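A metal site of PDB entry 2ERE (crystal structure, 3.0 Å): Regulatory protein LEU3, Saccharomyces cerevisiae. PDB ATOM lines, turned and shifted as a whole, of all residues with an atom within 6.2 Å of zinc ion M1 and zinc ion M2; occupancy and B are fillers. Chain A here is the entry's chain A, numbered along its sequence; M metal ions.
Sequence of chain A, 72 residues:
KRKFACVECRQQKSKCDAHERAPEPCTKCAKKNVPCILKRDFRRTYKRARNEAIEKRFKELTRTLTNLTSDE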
ATOM      1  N   ALA A   5       1.614 -23.113 -21.223  1.00  0.00           N
ATOM      2  CA  ALA A   5       1.117 -22.315 -22.348  1.00  0.00           C
ATOM      3  C   ALA A   5       2.105 -21.262 -22.853  1.00  0.00           C
ATOM      4  O   ALA A   5       2.821 -20.614 -22.070  1.00  0.00           O
ATOM      5  CB  ALA A   5      -0.203 -21.651 -21.956  1.00  0.00           C
ATOM      6  N   CYS A   6       2.157 -21.096 -24.176  1.00  0.00           N
ATOM      7  CA  CYS A   6       3.055 -20.127 -24.774  1.00  0.00           C
ATOM      8  C   CYS A   6       2.497 -18.736 -24.537  1.00  0.00           C
ATOM      9  O   CYS A   6       1.297 -18.553 -24.401  1.00  0.00           O
ATOM     10  CB  CYS A   6       3.197 -20.362 -26.277  1.00  0.00           C
ATOM     11  SG  CYS A   6       1.736 -20.017 -27.233  1.00  0.00           S
ATOM     12  N   VAL A   7       3.385 -17.755 -24.503  1.00  0.00           N
ATOM     13  CA  VAL A   7       2.958 -16.388 -24.235  1.00  0.00           C
ATOM     14  C   VAL A   7       1.750 -15.939 -25.042  1.00  0.00           C
ATOM     15  O   VAL A   7       0.766 -15.463 -24.472  1.00  0.00           O
ATOM     16  CB  VAL A   7       4.087 -15.398 -24.492  1.00  0.00           C
ATOM     17  CG1 VAL A   7       3.748 -14.065 -23.871  1.00  0.00           C
ATOM     18  CG2 VAL A   7       5.362 -15.936 -23.902  1.00  0.00           C
ATOM     19  N   GLU A   8       1.812 -16.094 -26.359  1.00  0.00           N
ATOM     20  CA  GLU A   8       0.718 -15.674 -27.230  1.00  0.00           C
ATOM     21  C   GLU A   8      -0.637 -16.333 -26.931  1.00  0.00           C
ATOM     22  O   GLU A   8      -1.672 -15.654 -26.853  1.00  0.00           O
ATOM     23  CB  GLU A   8       1.114 -15.918 -28.697  1.00  0.00           C
ATOM     24  CG  GLU A   8       0.190 -15.238 -29.726  1.00  0.00           C
ATOM     25  CD  GLU A   8       0.114 -13.725 -29.534  1.00  0.00           C
ATOM     26  OE1 GLU A   8       1.123 -13.127 -29.086  1.00  0.00           O
ATOM     27  OE2 GLU A   8      -0.951 -13.136 -29.855  1.00  0.00           O
ATOM     28  N   CYS A   9      -0.624 -17.659 -26.776  1.00  0.00           N
ATOM     29  CA  CYS A   9      -1.839 -18.411 -26.490  1.00  0.00           C
ATOM     30  C   CYS A   9      -2.443 -17.957 -25.175  1.00  0.00           C
ATOM     31  O   CYS A   9      -3.661 -17.866 -25.042  1.00  0.00           O
ATOM     32  CB  CYS A   9      -1.548 -19.908 -26.434  1.00  0.00           C
ATOM     33  SG  CYS A   9      -1.392 -20.730 -28.042  1.00  0.00           S
ATOM     34  N   ARG A  10      -1.584 -17.676 -24.202  1.00  0.00           N
ATOM     35  CA  ARG A  10      -2.021 -17.211 -22.896  1.00  0.00           C
ATOM     36  C   ARG A  10      -2.774 -15.919 -23.066  1.00  0.00           C
ATOM     37  O   ARG A  10      -3.770 -15.668 -22.387  1.00  0.00           O
ATOM     38  CB  ARG A  10      -0.836 -16.970 -21.961  1.00  0.00           C
ATOM     39  CG  ARG A  10      -0.277 -18.217 -21.356  1.00  0.00           C
ATOM     40  CD  ARG A  10       0.624 -17.906 -20.183  1.00  0.00           C
ATOM     41  NE  ARG A  10       0.973 -19.117 -19.455  1.00  0.00           N
ATOM     42  CZ  ARG A  10       1.842 -19.152 -18.452  1.00  0.00           C
ATOM     43  NH1 ARG A  10       2.432 -18.041 -18.068  1.00  0.00           N
ATOM     44  NH2 ARG A  10       2.121 -20.304 -17.856  1.00  0.00           N
ATOM     45  N   SER A  14      -5.996 -19.243 -25.665  1.00  0.00           N
ATOM     46  CA  SER A  14      -6.388 -20.285 -26.591  1.00  0.00           C
ATOM     47  C   SER A  14      -5.661 -21.580 -26.254  1.00  0.00           C
ATOM     48  O   SER A  14      -4.586 -21.534 -25.644  1.00  0.00           O
ATOM     49  CB  SER A  14      -6.009 -19.883 -27.998  1.00  0.00           C
ATOM     50  OG  SER A  14      -4.604 -19.807 -28.060  1.00  0.00           O
ATOM     51  N   LYS A  15      -6.232 -22.714 -26.644  1.00  0.00           N
ATOM     52  CA  LYS A  15      -5.584 -23.997 -26.388  1.00  0.00           C
ATOM     53  C   LYS A  15      -4.215 -23.878 -27.048  1.00  0.00           C
ATOM     54  O   LYS A  15      -4.127 -23.435 -28.187  1.00  0.00           O
ATOM     55  CB  LYS A  15      -6.367 -25.115 -27.015  1.00  0.00           C
ATOM     56  N   CYS A  16      -3.157 -24.260 -26.333  1.00  0.00           N
ATOM     57  CA  CYS A  16      -1.789 -24.192 -26.866  1.00  0.00           C
ATOM     58  C   CYS A  16      -1.132 -25.565 -26.924  1.00  0.00           C
ATOM     59  O   CYS A  16      -1.140 -26.292 -25.927  1.00  0.00           O
ATOM     60  CB  CYS A  16      -0.917 -23.283 -26.008  1.00  0.00           C
ATOM     61  SG  CYS A  16       0.825 -23.282 -26.480  1.00  0.00           S
ATOM     62  N   ASP A  17      -0.576 -25.923 -28.089  1.00  0.00           N
ATOM     63  CA  ASP A  17       0.052 -27.222 -28.239  1.00  0.00           C
ATOM     64  C   ASP A  17       1.554 -27.081 -28.361  1.00  0.00           C
ATOM     65  O   ASP A  17       2.066 -27.076 -29.471  1.00  0.00           O
ATOM     66  CB  ASP A  17      -0.496 -27.940 -29.456  1.00  0.00           C
ATOM     67  N   ALA A  18       2.248 -26.965 -27.229  1.00  0.00           N
ATOM     68  CA  ALA A  18       3.697 -26.845 -27.223  1.00  0.00           C
ATOM     69  C   ALA A  18       4.336 -27.976 -26.410  1.00  0.00           C
ATOM     70  O   ALA A  18       4.439 -29.119 -26.867  1.00  0.00           O
ATOM     71  CB  ALA A  18       4.107 -25.481 -26.658  1.00  0.00           C
ATOM     72  N   PRO A  25       7.743 -24.121 -32.096  1.00  0.00           N
ATOM     73  CA  PRO A  25       6.689 -23.112 -31.988  1.00  0.00           C
ATOM     74  C   PRO A  25       5.289 -23.727 -32.025  1.00  0.00           C
ATOM     75  O   PRO A  25       5.007 -24.590 -32.872  1.00  0.00           O
ATOM     76  CB  PRO A  25       6.967 -22.209 -33.191  1.00  0.00           C
ATOM     77  CG  PRO A  25       8.459 -22.221 -33.223  1.00  0.00           C
ATOM     78  CD  PRO A  25       8.795 -23.696 -33.033  1.00  0.00           C
ATOM     79  N   CYS A  26       4.427 -23.302 -31.102  1.00  0.00           N
ATOM     80  CA  CYS A  26       3.084 -23.850 -31.009  1.00  0.00           C
ATOM     81  C   CYS A  26       2.341 -23.638 -32.312  1.00  0.00           C
ATOM     82  O   CYS A  26       2.723 -22.783 -33.105  1.00  0.00           O
ATOM     83  CB  CYS A  26       2.312 -23.222 -29.854  1.00  0.00           C
ATOM     84  SG  CYS A  26       1.665 -21.585 -30.240  1.00  0.00           S
ATOM     85  N   THR A  27       1.280 -24.415 -32.508  1.00  0.00           N
ATOM     86  CA  THR A  27       0.465 -24.351 -33.736  1.00  0.00           C
ATOM     87  C   THR A  27      -0.034 -22.939 -34.082  1.00  0.00           C
ATOM     88  O   THR A  27       0.269 -22.395 -35.138  1.00  0.00           O
ATOM     89  CB  THR A  27      -0.756 -25.276 -33.602  1.00  0.00           C
ATOM     90  OG1 THR A  27      -0.313 -26.573 -33.170  1.00  0.00           O
ATOM     91  CG2 THR A  27      -1.485 -25.378 -34.950  1.00  0.00           C
ATOM     92  N   LYS A  28      -0.818 -22.362 -33.180  1.00  0.00           N
ATOM     93  CA  LYS A  28      -1.348 -21.024 -33.385  1.00  0.00           C
ATOM     94  C   LYS A  28      -0.254 -20.062 -33.829  1.00  0.00           C
ATOM     95  O   LYS A  28      -0.395 -19.405 -34.858  1.00  0.00           O
ATOM     96  CB  LYS A  28      -1.994 -20.524 -32.103  1.00  0.00           C
ATOM     97  CG  LYS A  28      -3.207 -21.337 -31.649  1.00  0.00           C
ATOM     98  CD  LYS A  28      -4.336 -21.350 -32.684  1.00  0.00           C
ATOM     99  CE  LYS A  28      -5.676 -21.717 -32.054  1.00  0.00           C
ATOM    100  NZ  LYS A  28      -5.608 -22.940 -31.192  1.00  0.00           N
ATOM    101  N   CYS A  29       0.830 -19.973 -33.061  1.00  0.00           N
ATOM    102  CA  CYS A  29       1.945 -19.082 -33.402  1.00  0.00           C
ATOM    103  C   CYS A  29       2.463 -19.347 -34.809  1.00  0.00           C
ATOM    104  O   CYS A  29       3.338 -18.632 -35.296  1.00  0.00           O
ATOM    105  CB  CYS A  29       3.098 -19.242 -32.387  1.00  0.00           C
ATOM    106  SG  CYS A  29       2.865 -18.413 -30.796  1.00  0.00           S
ATOM    107  N   VAL A  34       4.909 -15.986 -35.390  1.00  0.00           N
ATOM    108  CA  VAL A  34       5.426 -15.015 -34.440  1.00  0.00           C
ATOM    109  C   VAL A  34       6.283 -15.716 -33.414  1.00  0.00           C
ATOM    110  O   VAL A  34       6.246 -16.945 -33.285  1.00  0.00           O
ATOM    111  CB  VAL A  34       4.286 -14.282 -33.709  1.00  0.00           C
ATOM    112  CG1 VAL A  34       3.358 -13.629 -34.724  1.00  0.00           C
ATOM    113  CG2 VAL A  34       3.533 -15.268 -32.839  1.00  0.00           C
ATOM    114  N   PRO A  35       7.082 -14.942 -32.685  1.00  0.00           N
ATOM    115  CA  PRO A  35       7.953 -15.469 -31.640  1.00  0.00           C
ATOM    116  C   PRO A  35       7.191 -16.247 -30.551  1.00  0.00           C
ATOM    117  O   PRO A  35       6.614 -15.651 -29.625  1.00  0.00           O
ATOM    118  CB  PRO A  35       8.623 -14.213 -31.109  1.00  0.00           C
ATOM    119  CG  PRO A  35       8.807 -13.401 -32.355  1.00  0.00           C
ATOM    120  CD  PRO A  35       7.530 -13.611 -33.142  1.00  0.00           C
ATOM    121  N   CYS A  36       7.206 -17.571 -30.647  1.00  0.00           N
ATOM    122  CA  CYS A  36       6.543 -18.411 -29.675  1.00  0.00           C
ATOM    123  C   CYS A  36       7.383 -18.547 -28.401  1.00  0.00           C
ATOM    124  O   CYS A  36       8.092 -19.542 -28.207  1.00  0.00           O
ATOM    125  CB  CYS A  36       6.290 -19.782 -30.259  1.00  0.00           C
ATOM    126  SG  CYS A  36       5.569 -20.870 -29.061  1.00  0.00           S
ATOM    127  N   ILE A  37       7.295 -17.547 -27.530  1.00  0.00           N
ATOM    128  CA  ILE A  37       8.044 -17.564 -26.289  1.00  0.00           C
ATOM    129  C   ILE A  37       7.371 -18.454 -25.248  1.00  0.00           C
ATOM    130  O   ILE A  37       6.160 -18.691 -25.292  1.00  0.00           O
ATOM    131  CB  ILE A  37       8.214 -16.147 -25.764  1.00  0.00           C
ATOM    132  N   LEU A  38       8.171 -18.969 -24.313  1.00  0.00           N
ATOM    133  CA  LEU A  38       7.681 -19.806 -23.240  1.00  0.00           C
ATOM    134  C   LEU A  38       8.114 -19.122 -21.949  1.00  0.00           C
ATOM    135  O   LEU A  38       9.124 -19.503 -21.377  1.00  0.00           O
ATOM    136  CB  LEU A  38       8.294 -21.196 -23.321  1.00  0.00           C
ATOM    137  CG  LEU A  38       7.730 -22.180 -24.340  1.00  0.00           C
ATOM    138  CD1 LEU A  38       6.424 -22.744 -23.837  1.00  0.00           C
ATOM    139  CD2 LEU A  38       7.554 -21.500 -25.684  1.00  0.00           C
HETATM  140 ZN    ZN M   1       3.152 -20.343 -29.326  1.00  0.00          ZN
HETATM  141 ZN    ZN M   2       0.612 -21.763 -28.103  1.00  0.00          ZN
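The backbone carbonyl oxygen (O) of Cys 9 sits at hydrogen-bond distance from the backbone NH (N) of Ser 14, 2.8 Å away.
N of Val 34 is in hydrogen-bond range of O of Cys 29 (3.1 Å).
Of the 21 residues printed, 4 come within 4 Å of zinc ion M1.
The nearest printed residue that does not touch zinc ion M1 is Cys 16 (4.7 Å).
Within 4 Å of zinc ion M2: Cys 6, Cys 9, Cys 16 and Cys 26.
Zinc ion M1 is bound by the side-chain sulfur (SG) of Cys 26 (2.1 Å), the side-chain sulfur (SG) of Cys 29 (2.4 Å), the side-chain sulfur (SG) of Cys 36 (2.5 Å) and the side-chain sulfur (SG) of Cys 6 (2.5 Å).
Zinc ion M1 has four donor atoms within binding distance.
Zinc ion M2 is bound by SG of Cys 16 (2.2 Å), SG of Cys 6 (2.3 Å), SG of Cys 9 (2.3 Å) and SG of Cys 26 (2.4 Å).
Zinc ion M2 has four donor atoms within binding distance.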
